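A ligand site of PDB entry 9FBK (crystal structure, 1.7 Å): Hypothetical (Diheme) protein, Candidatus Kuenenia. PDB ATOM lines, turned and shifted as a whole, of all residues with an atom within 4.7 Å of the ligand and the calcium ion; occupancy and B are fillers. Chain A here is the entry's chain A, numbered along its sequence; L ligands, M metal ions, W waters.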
ATOM      1  N   ARG A  70       0.425  20.404   5.251  1.00  0.00           N
ATOM      2  CA  ARG A  70       1.403  21.257   5.946  1.00  0.00           C
ATOM      3  C   ARG A  70       1.147  21.309   7.450  1.00  0.00           C
ATOM      4  O   ARG A  70       2.087  21.394   8.240  1.00  0.00           O
ATOM      5  CB  ARG A  70       1.418  22.676   5.363  1.00  0.00           C
ATOM      6  CG  ARG A  70       2.223  22.813   4.064  1.00  0.00           C
ATOM      7  CD  ARG A  70       2.070  24.186   3.476  1.00  0.00           C
ATOM      8  NE  ARG A  70       2.827  24.342   2.239  1.00  0.00           N
ATOM      9  CZ  ARG A  70       2.365  23.985   1.048  1.00  0.00           C
ATOM     10  NH1 ARG A  70       1.154  23.463   0.898  1.00  0.00           N
ATOM     11  NH2 ARG A  70       3.137  24.154  -0.030  1.00  0.00           N
ATOM     12  N   ILE A 115       5.251  27.286  10.886  1.00  0.00           N
ATOM     13  CA  ILE A 115       4.827  27.694   9.548  1.00  0.00           C
ATOM     14  C   ILE A 115       3.434  28.353   9.566  1.00  0.00           C
ATOM     15  O   ILE A 115       3.138  29.150   8.650  1.00  0.00           O
ATOM     16  CB  ILE A 115       4.868  26.470   8.601  1.00  0.00           C
ATOM     17  CG1 ILE A 115       4.709  26.848   7.120  1.00  0.00           C
ATOM     18  CG2 ILE A 115       3.816  25.496   8.937  1.00  0.00           C
ATOM     19  CD1 ILE A 115       4.804  25.627   6.203  1.00  0.00           C
ATOM     20  N   PHE A 183      13.042  33.699 -10.962  1.00  0.00           N
ATOM     21  CA  PHE A 183      12.616  32.408 -10.421  1.00  0.00           C
ATOM     22  C   PHE A 183      12.902  31.265 -11.401  1.00  0.00           C
ATOM     23  O   PHE A 183      13.289  30.164 -10.981  1.00  0.00           O
ATOM     24  CB  PHE A 183      11.128  32.496 -10.093  1.00  0.00           C
ATOM     25  CG  PHE A 183      10.558  31.340  -9.308  1.00  0.00           C
ATOM     26  CD1 PHE A 183      10.159  30.168  -9.935  1.00  0.00           C
ATOM     27  CD2 PHE A 183      10.352  31.453  -7.947  1.00  0.00           C
ATOM     28  CE1 PHE A 183       9.590  29.120  -9.203  1.00  0.00           C
ATOM     29  CE2 PHE A 183       9.778  30.417  -7.212  1.00  0.00           C
ATOM     30  CZ  PHE A 183       9.401  29.256  -7.840  1.00  0.00           C
ATOM     31  N   VAL A 190      21.343  29.591  -8.851  1.00  0.00           N
ATOM     32  CA  VAL A 190      20.190  28.921  -8.266  1.00  0.00           C
ATOM     33  C   VAL A 190      18.988  29.227  -9.151  1.00  0.00           C
ATOM     34  O   VAL A 190      18.845  30.361  -9.637  1.00  0.00           O
ATOM     35  CB  VAL A 190      19.972  29.356  -6.799  1.00  0.00           C
ATOM     36  CG1 VAL A 190      19.695  30.836  -6.708  1.00  0.00           C
ATOM     37  CG2 VAL A 190      18.844  28.571  -6.177  1.00  0.00           C
ATOM     38  N   THR A 191      18.164  28.215  -9.401  1.00  0.00           N
ATOM     39  CA  THR A 191      16.967  28.392 -10.230  1.00  0.00           C
ATOM     40  C   THR A 191      15.817  27.783  -9.436  1.00  0.00           C
ATOM     41  O   THR A 191      15.722  26.552  -9.349  1.00  0.00           O
ATOM     42  CB  THR A 191      17.114  27.723 -11.608  1.00  0.00           C
ATOM     43  OG1 THR A 191      18.268  28.251 -12.274  1.00  0.00           O
ATOM     44  CG2 THR A 191      15.874  27.960 -12.476  1.00  0.00           C
ATOM     45  N   CYS A 192      14.974  28.634  -8.824  1.00  0.00           N
ATOM     46  CA  CYS A 192      13.876  28.109  -8.016  1.00  0.00           C
ATOM     47  C   CYS A 192      13.040  27.119  -8.803  1.00  0.00           C
ATOM     48  O   CYS A 192      12.571  26.109  -8.260  1.00  0.00           O
ATOM     49  CB  CYS A 192      12.966  29.234  -7.528  1.00  0.00           C
ATOM     50  SG  CYS A 192      13.840  30.688  -6.931  1.00  0.00           S
ATOM     51  N   CYS A 195      13.127  23.258  -8.761  1.00  0.00           N
ATOM     52  CA  CYS A 195      12.573  22.500  -7.649  1.00  0.00           C
ATOM     53  C   CYS A 195      11.138  22.869  -7.295  1.00  0.00           C
ATOM     54  O   CYS A 195      10.517  22.147  -6.494  1.00  0.00           O
ATOM     55  CB  CYS A 195      13.438  22.691  -6.404  1.00  0.00           C
ATOM     56  SG  CYS A 195      15.102  21.968  -6.500  1.00  0.00           S
ATOM     57  N   HIS A 196      10.586  23.924  -7.856  1.00  0.00           N
ATOM     58  CA  HIS A 196       9.270  24.398  -7.471  1.00  0.00           C
ATOM     59  C   HIS A 196       8.441  24.667  -8.712  1.00  0.00           C
ATOM     60  O   HIS A 196       8.930  25.262  -9.683  1.00  0.00           O
ATOM     61  CB  HIS A 196       9.346  25.697  -6.662  1.00  0.00           C
ATOM     62  CG  HIS A 196       9.921  25.528  -5.292  1.00  0.00           C
ATOM     63  ND1 HIS A 196       9.203  24.986  -4.244  1.00  0.00           N
ATOM     64  CD2 HIS A 196      11.129  25.870  -4.787  1.00  0.00           C
ATOM     65  CE1 HIS A 196       9.935  25.012  -3.150  1.00  0.00           C
ATOM     66  NE2 HIS A 196      11.114  25.521  -3.452  1.00  0.00           N
ATOM     67  N   VAL A 205      10.186  19.267  -6.935  1.00  0.00           N
ATOM     68  CA  VAL A 205      11.111  18.666  -5.975  1.00  0.00           C
ATOM     69  C   VAL A 205      10.633  19.080  -4.575  1.00  0.00           C
ATOM     70  O   VAL A 205      10.257  18.244  -3.750  1.00  0.00           O
ATOM     71  CB  VAL A 205      12.573  19.099  -6.199  1.00  0.00           C
ATOM     72  CG1 VAL A 205      13.460  18.491  -5.142  1.00  0.00           C
ATOM     73  CG2 VAL A 205      13.103  18.681  -7.583  1.00  0.00           C
ATOM     74  N   GLY A 206      10.644  20.387  -4.310  1.00  0.00           N
ATOM     75  CA  GLY A 206       9.926  20.930  -3.173  1.00  0.00           C
ATOM     76  C   GLY A 206       8.463  21.152  -3.492  1.00  0.00           C
ATOM     77  O   GLY A 206       7.982  20.863  -4.593  1.00  0.00           O
ATOM     78  N   PRO A 207       7.731  21.727  -2.536  1.00  0.00           N
ATOM     79  CA  PRO A 207       6.282  21.886  -2.714  1.00  0.00           C
ATOM     80  C   PRO A 207       5.913  22.895  -3.811  1.00  0.00           C
ATOM     81  O   PRO A 207       6.662  23.821  -4.136  1.00  0.00           O
ATOM     82  CB  PRO A 207       5.806  22.370  -1.333  1.00  0.00           C
ATOM     83  CG  PRO A 207       7.051  22.970  -0.692  1.00  0.00           C
ATOM     84  CD  PRO A 207       8.180  22.126  -1.196  1.00  0.00           C
ATOM     85  N   LEU A 209       4.341  26.103  -5.251  1.00  0.00           N
ATOM     86  CA  LEU A 209       4.244  27.398  -4.610  1.00  0.00           C
ATOM     87  C   LEU A 209       3.041  28.202  -5.080  1.00  0.00           C
ATOM     88  O   LEU A 209       2.805  29.292  -4.561  1.00  0.00           O
ATOM     89  CB  LEU A 209       5.538  28.207  -4.801  1.00  0.00           C
ATOM     90  CG  LEU A 209       6.772  27.584  -4.147  1.00  0.00           C
ATOM     91  CD1 LEU A 209       7.980  28.548  -4.321  1.00  0.00           C
ATOM     92  CD2 LEU A 209       6.523  27.225  -2.679  1.00  0.00           C
ATOM     93  N   ILE A 212       0.851  30.727  -2.669  1.00  0.00           N
ATOM     94  CA  ILE A 212       1.442  30.949  -1.345  1.00  0.00           C
ATOM     95  C   ILE A 212       1.456  32.430  -1.000  1.00  0.00           C
ATOM     96  O   ILE A 212       1.474  32.788   0.185  1.00  0.00           O
ATOM     97  CB  ILE A 212       2.846  30.312  -1.296  1.00  0.00           C
ATOM     98  CG1 ILE A 212       3.321  30.103   0.150  1.00  0.00           C
ATOM     99  CG2 ILE A 212       3.865  31.113  -2.156  1.00  0.00           C
ATOM    100  CD1 ILE A 212       4.710  29.414   0.228  1.00  0.00           C
ATOM    101  N   TYR A 220       8.316  35.254   6.150  1.00  0.00           N
ATOM    102  CA  TYR A 220       8.441  33.806   5.917  1.00  0.00           C
ATOM    103  C   TYR A 220       9.183  33.501   4.609  1.00  0.00           C
ATOM    104  O   TYR A 220       9.974  32.551   4.534  1.00  0.00           O
ATOM    105  CB  TYR A 220       7.061  33.121   5.933  1.00  0.00           C
ATOM    106  CG  TYR A 220       7.148  31.626   5.650  1.00  0.00           C
ATOM    107  CD1 TYR A 220       7.574  30.751   6.614  1.00  0.00           C
ATOM    108  CD2 TYR A 220       6.790  31.121   4.411  1.00  0.00           C
ATOM    109  CE1 TYR A 220       7.662  29.398   6.371  1.00  0.00           C
ATOM    110  CE2 TYR A 220       6.882  29.767   4.144  1.00  0.00           C
ATOM    111  CZ  TYR A 220       7.320  28.908   5.139  1.00  0.00           C
ATOM    112  OH  TYR A 220       7.402  27.550   4.908  1.00  0.00           O
ATOM    113  N   PHE A 221       8.940  34.297   3.557  1.00  0.00           N
ATOM    114  CA  PHE A 221       9.705  34.066   2.328  1.00  0.00           C
ATOM    115  C   PHE A 221      11.181  34.351   2.568  1.00  0.00           C
ATOM    116  O   PHE A 221      12.035  33.585   2.103  1.00  0.00           O
ATOM    117  CB  PHE A 221       9.172  34.900   1.171  1.00  0.00           C
ATOM    118  CG  PHE A 221       7.694  34.640   0.847  1.00  0.00           C
ATOM    119  CD1 PHE A 221       7.172  33.346   0.934  1.00  0.00           C
ATOM    120  CD2 PHE A 221       6.863  35.668   0.474  1.00  0.00           C
ATOM    121  CE1 PHE A 221       5.830  33.098   0.661  1.00  0.00           C
ATOM    122  CE2 PHE A 221       5.530  35.433   0.202  1.00  0.00           C
ATOM    123  CZ  PHE A 221       5.010  34.163   0.292  1.00  0.00           C
ATOM    124  N   SER A 224      12.488  31.428   4.438  1.00  0.00           N
ATOM    125  CA  SER A 224      12.504  30.231   3.610  1.00  0.00           C
ATOM    126  C   SER A 224      13.688  30.238   2.663  1.00  0.00           C
ATOM    127  O   SER A 224      14.260  29.188   2.387  1.00  0.00           O
ATOM    128  CB  SER A 224      11.203  30.132   2.808  1.00  0.00           C
ATOM    129  OG  SER A 224      10.153  29.667   3.625  1.00  0.00           O
ATOM    130  N   ILE A 225      14.075  31.415   2.162  1.00  0.00           N
ATOM    131  CA  ILE A 225      15.139  31.511   1.167  1.00  0.00           C
ATOM    132  C   ILE A 225      16.507  31.492   1.848  1.00  0.00           C
ATOM    133  O   ILE A 225      17.412  30.775   1.414  1.00  0.00           O
ATOM    134  CB  ILE A 225      14.967  32.763   0.291  1.00  0.00           C
ATOM    135  CG1 ILE A 225      13.663  32.647  -0.478  1.00  0.00           C
ATOM    136  CG2 ILE A 225      16.210  32.962  -0.650  1.00  0.00           C
ATOM    137  CD1 ILE A 225      13.243  33.946  -1.151  1.00  0.00           C
ATOM    138  N   PRO A 228      16.733  27.868   4.978  1.00  0.00           N
ATOM    139  CA  PRO A 228      15.770  26.886   4.472  1.00  0.00           C
ATOM    140  C   PRO A 228      15.461  25.767   5.426  1.00  0.00           C
ATOM    141  O   PRO A 228      14.376  25.173   5.291  1.00  0.00           O
ATOM    142  CB  PRO A 228      16.412  26.356   3.181  1.00  0.00           C
ATOM    143  CG  PRO A 228      17.946  26.648   3.368  1.00  0.00           C
ATOM    144  CD  PRO A 228      17.919  27.983   4.089  1.00  0.00           C
ATOM    145  N   SER A 229      16.335  25.435   6.388  1.00  0.00           N
ATOM    146  CA  SER A 229      16.041  24.360   7.318  1.00  0.00           C
ATOM    147  C   SER A 229      15.373  24.840   8.598  1.00  0.00           C
ATOM    148  O   SER A 229      15.037  24.026   9.445  1.00  0.00           O
ATOM    149  CB  SER A 229      17.314  23.577   7.653  1.00  0.00           C
ATOM    150  OG  SER A 229      17.935  23.035   6.492  1.00  0.00           O
ATOM    151  N   VAL A 231      12.352  25.979   8.852  1.00  0.00           N
ATOM    152  CA  VAL A 231      11.062  25.338   8.710  1.00  0.00           C
ATOM    153  C   VAL A 231      11.217  24.307   7.592  1.00  0.00           C
ATOM    154  O   VAL A 231      11.758  24.620   6.529  1.00  0.00           O
ATOM    155  CB  VAL A 231       9.962  26.356   8.356  1.00  0.00           C
ATOM    156  CG1 VAL A 231       8.673  25.641   7.932  1.00  0.00           C
ATOM    157  CG2 VAL A 231       9.683  27.309   9.494  1.00  0.00           C
ATOM    158  N   ILE A 232      10.772  23.076   7.850  1.00  0.00           N
ATOM    159  CA  ILE A 232      10.731  22.019   6.834  1.00  0.00           C
ATOM    160  C   ILE A 232       9.267  21.736   6.576  1.00  0.00           C
ATOM    161  O   ILE A 232       8.575  21.239   7.469  1.00  0.00           O
ATOM    162  CB  ILE A 232      11.435  20.752   7.308  1.00  0.00           C
ATOM    163  CG1 ILE A 232      12.874  21.066   7.739  1.00  0.00           C
ATOM    164  CG2 ILE A 232      11.335  19.648   6.197  1.00  0.00           C
ATOM    165  CD1 ILE A 232      13.819  21.378   6.593  1.00  0.00           C
ATOM    166  N   VAL A 233       8.790  22.066   5.373  1.00  0.00           N
ATOM    167  CA  VAL A 233       7.409  21.749   5.005  1.00  0.00           C
ATOM    168  C   VAL A 233       7.171  20.256   5.191  1.00  0.00           C
ATOM    169  O   VAL A 233       7.993  19.412   4.794  1.00  0.00           O
ATOM    170  CB  VAL A 233       7.131  22.191   3.560  1.00  0.00           C
ATOM    171  CG1 VAL A 233       5.663  21.852   3.146  1.00  0.00           C
ATOM    172  CG2 VAL A 233       7.434  23.698   3.380  1.00  0.00           C
ATOM    173  N   TYR A 236       8.573  16.864   3.267  1.00  0.00           N
ATOM    174  CA  TYR A 236       9.720  17.200   2.441  1.00  0.00           C
ATOM    175  C   TYR A 236      11.002  17.155   3.246  1.00  0.00           C
ATOM    176  O   TYR A 236      11.957  17.881   2.970  1.00  0.00           O
ATOM    177  CB  TYR A 236       9.542  18.561   1.784  1.00  0.00           C
ATOM    178  CG  TYR A 236       8.445  18.596   0.761  1.00  0.00           C
ATOM    179  CD1 TYR A 236       7.143  18.896   1.135  1.00  0.00           C
ATOM    180  CD2 TYR A 236       8.699  18.317  -0.574  1.00  0.00           C
ATOM    181  CE1 TYR A 236       6.122  18.940   0.198  1.00  0.00           C
ATOM    182  CE2 TYR A 236       7.676  18.355  -1.522  1.00  0.00           C
ATOM    183  CZ  TYR A 236       6.387  18.661  -1.114  1.00  0.00           C
ATOM    184  OH  TYR A 236       5.361  18.696  -2.021  1.00  0.00           O
ATOM    185  N   LEU A 252      15.449  13.755  -0.157  1.00  0.00           N
ATOM    186  CA  LEU A 252      14.023  13.694   0.187  1.00  0.00           C
ATOM    187  C   LEU A 252      13.346  12.555  -0.561  1.00  0.00           C
ATOM    188  O   LEU A 252      13.803  12.103  -1.611  1.00  0.00           O
ATOM    189  CB  LEU A 252      13.329  15.028  -0.090  1.00  0.00           C
ATOM    190  CG  LEU A 252      13.017  15.653  -1.460  1.00  0.00           C
ATOM    191  CD1 LEU A 252      11.989  14.884  -2.254  1.00  0.00           C
ATOM    192  CD2 LEU A 252      12.515  17.082  -1.250  1.00  0.00           C
ATOM    193  N   GLU A 266      20.342  16.292  -3.713  1.00  0.00           N
ATOM    194  CA  GLU A 266      20.769  17.601  -4.151  1.00  0.00           C
ATOM    195  C   GLU A 266      22.267  17.742  -3.931  1.00  0.00           C
ATOM    196  O   GLU A 266      22.805  17.253  -2.931  1.00  0.00           O
ATOM    197  CB  GLU A 266      20.036  18.720  -3.403  1.00  0.00           C
ATOM    198  CG  GLU A 266      20.365  20.104  -3.917  1.00  0.00           C
ATOM    199  CD  GLU A 266      21.608  20.729  -3.249  1.00  0.00           C
ATOM    200  OE1 GLU A 266      22.009  20.271  -2.168  1.00  0.00           O
ATOM    201  OE2 GLU A 266      22.183  21.676  -3.826  1.00  0.00           O
ATOM    202  N   VAL A 271      19.843  18.486  -8.920  1.00  0.00           N
ATOM    203  CA  VAL A 271      19.093  17.399  -8.291  1.00  0.00           C
ATOM    204  C   VAL A 271      19.216  16.145  -9.140  1.00  0.00           C
ATOM    205  O   VAL A 271      19.410  16.212 -10.366  1.00  0.00           O
ATOM    206  CB  VAL A 271      17.612  17.759  -8.068  1.00  0.00           C
ATOM    207  CG1 VAL A 271      17.489  18.707  -6.826  1.00  0.00           C
ATOM    208  CG2 VAL A 271      16.966  18.393  -9.315  1.00  0.00           C
ATOM    209  N   SER A 290      17.068  20.699   5.095  1.00  0.00           N
ATOM    210  CA  SER A 290      16.297  20.789   3.854  1.00  0.00           C
ATOM    211  C   SER A 290      17.218  20.566   2.666  1.00  0.00           C
ATOM    212  O   SER A 290      18.400  20.918   2.699  1.00  0.00           O
ATOM    213  CB  SER A 290      15.622  22.165   3.753  1.00  0.00           C
ATOM    214  OG  SER A 290      14.884  22.281   2.541  1.00  0.00           O
ATOM    215  N   ILE A 291      16.687  19.954   1.591  1.00  0.00           N
ATOM    216  CA  ILE A 291      17.502  19.868   0.385  1.00  0.00           C
ATOM    217  C   ILE A 291      17.524  21.192  -0.367  1.00  0.00           C
ATOM    218  O   ILE A 291      18.405  21.380  -1.226  1.00  0.00           O
ATOM    219  CB  ILE A 291      17.110  18.744  -0.594  1.00  0.00           C
ATOM    220  CG1 ILE A 291      15.831  19.075  -1.319  1.00  0.00           C
ATOM    221  CG2 ILE A 291      17.022  17.403   0.098  1.00  0.00           C
ATOM    222  CD1 ILE A 291      15.620  18.141  -2.495  1.00  0.00           C
ATOM    223  N   MET A 292      16.643  22.125  -0.037  1.00  0.00           N
ATOM    224  CA  MET A 292      16.776  23.461  -0.606  1.00  0.00           C
ATOM    225  C   MET A 292      18.148  24.044  -0.242  1.00  0.00           C
ATOM    226  O   MET A 292      18.524  24.021   0.945  1.00  0.00           O
ATOM    227  CB  MET A 292      15.660  24.365  -0.094  1.00  0.00           C
ATOM    228  CG  MET A 292      15.717  25.786  -0.629  1.00  0.00           C
ATOM    229  SD  MET A 292      14.099  26.615  -0.410  1.00  0.00           S
ATOM    230  CE  MET A 292      14.554  28.355  -0.612  1.00  0.00           C
ATOM    231  N   PRO A 293      18.910  24.559  -1.211  1.00  0.00           N
ATOM    232  CA  PRO A 293      20.288  24.988  -0.931  1.00  0.00           C
ATOM    233  C   PRO A 293      20.383  26.008   0.190  1.00  0.00           C
ATOM    234  O   PRO A 293      19.551  26.914   0.310  1.00  0.00           O
ATOM    235  CB  PRO A 293      20.763  25.567  -2.268  1.00  0.00           C
ATOM    236  CG  PRO A 293      19.965  24.810  -3.282  1.00  0.00           C
ATOM    237  CD  PRO A 293      18.597  24.626  -2.647  1.00  0.00           C
ATOM    238  N   ILE A 296      21.794  30.389  -0.661  1.00  0.00           N
ATOM    239  CA  ILE A 296      21.182  31.233  -1.666  1.00  0.00           C
ATOM    240  C   ILE A 296      21.555  32.697  -1.461  1.00  0.00           C
ATOM    241  O   ILE A 296      21.641  33.453  -2.429  1.00  0.00           O
ATOM    242  CB  ILE A 296      19.661  30.970  -1.662  1.00  0.00           C
ATOM    243  CG1 ILE A 296      19.417  29.531  -2.149  1.00  0.00           C
ATOM    244  CG2 ILE A 296      18.946  31.955  -2.544  1.00  0.00           C
ATOM    245  CD1 ILE A 296      17.931  29.117  -1.955  1.00  0.00           C
ATOM    246  N   LEU A 300      22.233  34.859  -5.037  1.00  0.00           N
ATOM    247  CA  LEU A 300      21.387  35.905  -5.600  1.00  0.00           C
ATOM    248  C   LEU A 300      21.939  37.273  -5.225  1.00  0.00           C
ATOM    249  O   LEU A 300      22.390  37.487  -4.098  1.00  0.00           O
ATOM    250  CB  LEU A 300      19.953  35.801  -5.074  1.00  0.00           C
ATOM    251  CG  LEU A 300      19.232  34.497  -5.412  1.00  0.00           C
ATOM    252  CD1 LEU A 300      17.835  34.562  -4.817  1.00  0.00           C
ATOM    253  CD2 LEU A 300      19.204  34.309  -6.928  1.00  0.00           C
ATOM    254  N   VAL A 308      12.491  38.249  -6.330  1.00  0.00           N
ATOM    255  CA  VAL A 308      11.850  36.952  -6.117  1.00  0.00           C
ATOM    256  C   VAL A 308      10.809  37.066  -5.015  1.00  0.00           C
ATOM    257  O   VAL A 308       9.700  36.522  -5.140  1.00  0.00           O
ATOM    258  CB  VAL A 308      12.901  35.892  -5.782  1.00  0.00           C
ATOM    259  CG1 VAL A 308      12.219  34.598  -5.340  1.00  0.00           C
ATOM    260  CG2 VAL A 308      13.774  35.649  -6.943  1.00  0.00           C
ATOM    261  N   LEU A 312       6.914  35.935  -5.111  1.00  0.00           N
ATOM    262  CA  LEU A 312       6.171  35.049  -4.215  1.00  0.00           C
ATOM    263  C   LEU A 312       4.941  35.742  -3.634  1.00  0.00           C
ATOM    264  O   LEU A 312       3.871  35.129  -3.539  1.00  0.00           O
ATOM    265  CB  LEU A 312       7.084  34.547  -3.080  1.00  0.00           C
ATOM    266  CG  LEU A 312       8.273  33.701  -3.562  1.00  0.00           C
ATOM    267  CD1 LEU A 312       9.301  33.526  -2.442  1.00  0.00           C
ATOM    268  CD2 LEU A 312       7.778  32.367  -4.115  1.00  0.00           C
HETATM  269 FE1  LIG L   1      12.584  26.007  -2.120  1.00  0.00          FE
HETATM  270  C1  LIG L   1      10.613  25.100   0.432  1.00  0.00           C
HETATM  271  C2  LIG L   1      11.196  29.221  -2.003  1.00  0.00           C
HETATM  272  C3  LIG L   1      14.715  27.094  -4.646  1.00  0.00           C
HETATM  273  C4  LIG L   1      13.697  22.815  -2.601  1.00  0.00           C
HETATM  274  N1  LIG L   1      11.141  27.009  -0.994  1.00  0.00           N
HETATM  275  C5  LIG L   1      10.434  26.392   0.017  1.00  0.00           C
HETATM  276  C6  LIG L   1       9.477  27.374   0.552  1.00  0.00           C
HETATM  277  C7  LIG L   1       9.637  28.508  -0.129  1.00  0.00           C
HETATM  278  C8  LIG L   1      10.693  28.296  -1.113  1.00  0.00           C
HETATM  279  C9  LIG L   1       8.888  29.850  -0.009  1.00  0.00           C
HETATM  280  C10 LIG L   1       8.435  27.080   1.666  1.00  0.00           C
HETATM  281  C11 LIG L   1       7.201  26.542   0.905  1.00  0.00           C
HETATM  282  C12 LIG L   1       5.932  26.387   1.732  1.00  0.00           C
HETATM  283  O1  LIG L   1       4.941  25.734   1.259  1.00  0.00           O
HETATM  284  O2  LIG L   1       5.889  26.878   2.869  1.00  0.00           O
HETATM  285  N2  LIG L   1      12.894  27.769  -3.108  1.00  0.00           N
HETATM  286  C13 LIG L   1      12.240  28.967  -2.892  1.00  0.00           C
HETATM  287  C14 LIG L   1      12.876  29.982  -3.691  1.00  0.00           C
HETATM  288  C15 LIG L   1      13.795  29.402  -4.475  1.00  0.00           C
HETATM  289  C16 LIG L   1      13.855  28.014  -4.096  1.00  0.00           C
HETATM  290  C17 LIG L   1      12.296  31.419  -3.758  1.00  0.00           C
HETATM  291  C18 LIG L   1      14.700  30.055  -5.522  1.00  0.00           C
HETATM  292  C19 LIG L   1      15.541  31.223  -4.960  1.00  0.00           C
HETATM  293  N3  LIG L   1      13.958  25.108  -3.398  1.00  0.00           N
HETATM  294  C20 LIG L   1      14.723  25.750  -4.359  1.00  0.00           C
HETATM  295  C21 LIG L   1      15.650  24.782  -4.912  1.00  0.00           C
HETATM  296  C22 LIG L   1      15.283  23.569  -4.460  1.00  0.00           C
HETATM  297  C23 LIG L   1      14.263  23.777  -3.417  1.00  0.00           C
HETATM  298  C24 LIG L   1      16.547  25.074  -6.145  1.00  0.00           C
HETATM  299  C25 LIG L   1      15.824  22.179  -4.881  1.00  0.00           C
HETATM  300  C26 LIG L   1      17.337  21.895  -4.795  1.00  0.00           C
HETATM  301  N4  LIG L   1      12.250  24.224  -1.197  1.00  0.00           N
HETATM  302  C27 LIG L   1      12.811  23.016  -1.568  1.00  0.00           C
HETATM  303  C28 LIG L   1      12.281  22.005  -0.670  1.00  0.00           C
HETATM  304  C29 LIG L   1      11.326  22.704   0.261  1.00  0.00           C
HETATM  305  C30 LIG L   1      11.348  24.088  -0.146  1.00  0.00           C
HETATM  306  C31 LIG L   1      12.597  20.505  -0.622  1.00  0.00           C
HETATM  307  C32 LIG L   1      10.563  21.988   1.387  1.00  0.00           C
HETATM  308  C33 LIG L   1      11.492  21.859   2.597  1.00  0.00           C
HETATM  309  C34 LIG L   1      11.733  23.220   3.220  1.00  0.00           C
HETATM  310  O3  LIG L   1      10.801  23.772   3.813  1.00  0.00           O
HETATM  311  O4  LIG L   1      12.866  23.756   3.105  1.00  0.00           O
HETATM  312 CA    CA M   1      12.184  25.613   4.635  1.00  0.00          CA
HETATM  313  O   HOH W   1       3.371  27.720   3.634  1.00  0.00           O
HETATM  314  O   HOH W   2      12.850  27.436   5.986  1.00  0.00           O
HETATM  315  O   HOH W   3      10.221  27.120   4.614  1.00  0.00           O
HETATM  316  O   HOH W   4      12.832  26.929   2.606  1.00  0.00           O
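The side-chain sulfur (SG) of Cys 192 is bonded to a carbon (C18) of the ligand (1.8 Å).
The side-chain sulfur (SG) of Cys 195 is covalently linked to a carbon (C25) of the ligand, at 1.8 Å.
A ring nitrogen (NE2) of His 196 is bound to an iron atom (FE1) of the ligand, 2.0 Å away.
SD of Met 292 binds FE1 of the ligand (2.4 Å).
O4 of the ligand lies close to OG of Ser 290, 2.6 Å away.
The side-chain hydroxyl (OH) of Tyr 220 is in hydrogen-bond range of an oxygen (O2) of the ligand (2.6 Å).
NE of Arg 70 is in salt-bridge range of O1 of the ligand (2.7 Å).
An oxygen (O3) of the ligand lies close to the backbone NH of Val 233, 3.1 Å away.
O of Phe 183 is in hydrogen-bond range of N of Cys 192 (3.1 Å).
The backbone carbonyl oxygen (O) of Cys 195 lies within hydrogen-bond range of the backbone NH (N) of Gly 206 (2.8 Å).
The backbone carbonyl oxygen (O) of Cys 195 sits at hydrogen-bond distance from the backbone NH (N) of Val 205 (2.9 Å).
A ring nitrogen (ND1) of His 196 is in hydrogen-bond range of the backbone carbonyl oxygen (O) of Pro 207 (2.8 Å).
The backbone NH of Met 292 is in hydrogen-bond range of the side-chain hydroxyl of Ser 290 (3.1 Å).
N of Ser 290 lies within hydrogen-bond range of OG of Ser 229 (2.9 Å).
O of Tyr 220 sits at hydrogen-bond distance from OG of Ser 224 (3.0 Å).
Ile 115 touches the ligand (CD1 to O2, 3.7 Å).
Thr 191 touches the ligand (O to C24, 3.6 Å).
CA of Gly 206 touches C28 of the ligand, 3.6 Å away.
Pro 207 touches the ligand.
Leu 209 touches the ligand.
Ile 212 touches the ligand.
Ser 224 touches the ligand.
Ile 225 touches the ligand.
Ile 232 touches the ligand (CA to O3, 3.5 Å).
Tyr 236 touches the ligand.
Leu 252 touches the ligand.
CG of Glu 266 touches C26 of the ligand (3.6 Å).
CG1 of Val 271 touches C26 of the ligand, at 3.8 Å.
Ile 291 touches the ligand (CG1 to C31, 3.6 Å).
Pro 293 touches the ligand.
CG1 of Val 308 touches C17 of the ligand (3.6 Å).
Leu 312 touches the ligand.
Hydrophobic or aromatic side chains within 4 Å of the ligand: Ile 115, His 196, Pro 207, Leu 209, Ile 212, Tyr 220, Ile 225, Val 233, Tyr 236, Leu 252, Val 271, Ile 291, Met 292, Pro 293, Val 308 and Leu 312.
27 residues have an atom within 4 Å of the ligand: Arg 70, Ile 115, Thr 191, Cys 192, Cys 195, His 196, Gly 206, Pro 207, Leu 209, Ile 212, Tyr 220, Ser 224, Ile 225, Pro 228, Val 231, Ile 232, Val 233, Tyr 236, Leu 252, Glu 266, Val 271, Ser 290, Ile 291, Met 292, Pro 293, Val 308 and Leu 312.
Within 4 Å of the calcium ion: Pro 228 and Val 231.
Along chain A the residues within 4 Å of the calcium ion span positions 228 to 231.
The calcium ion is bound by the backbone carbonyl oxygen of Val 231 (2.2 Å), the backbone carbonyl oxygen of Pro 228 (2.3 Å), water W2 (2.4 Å), an oxygen (O3) of the ligand (2.4 Å), water W3 (2.5 Å), an oxygen (O4) of the ligand (2.5 Å) and water W4 (2.5 Å).
The calcium ion has seven donor atoms within binding distance.
Water W3 lies within hydrogen-bond range of OG of Ser 224 (2.7 Å) and OH of Tyr 220 (2.9 Å).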
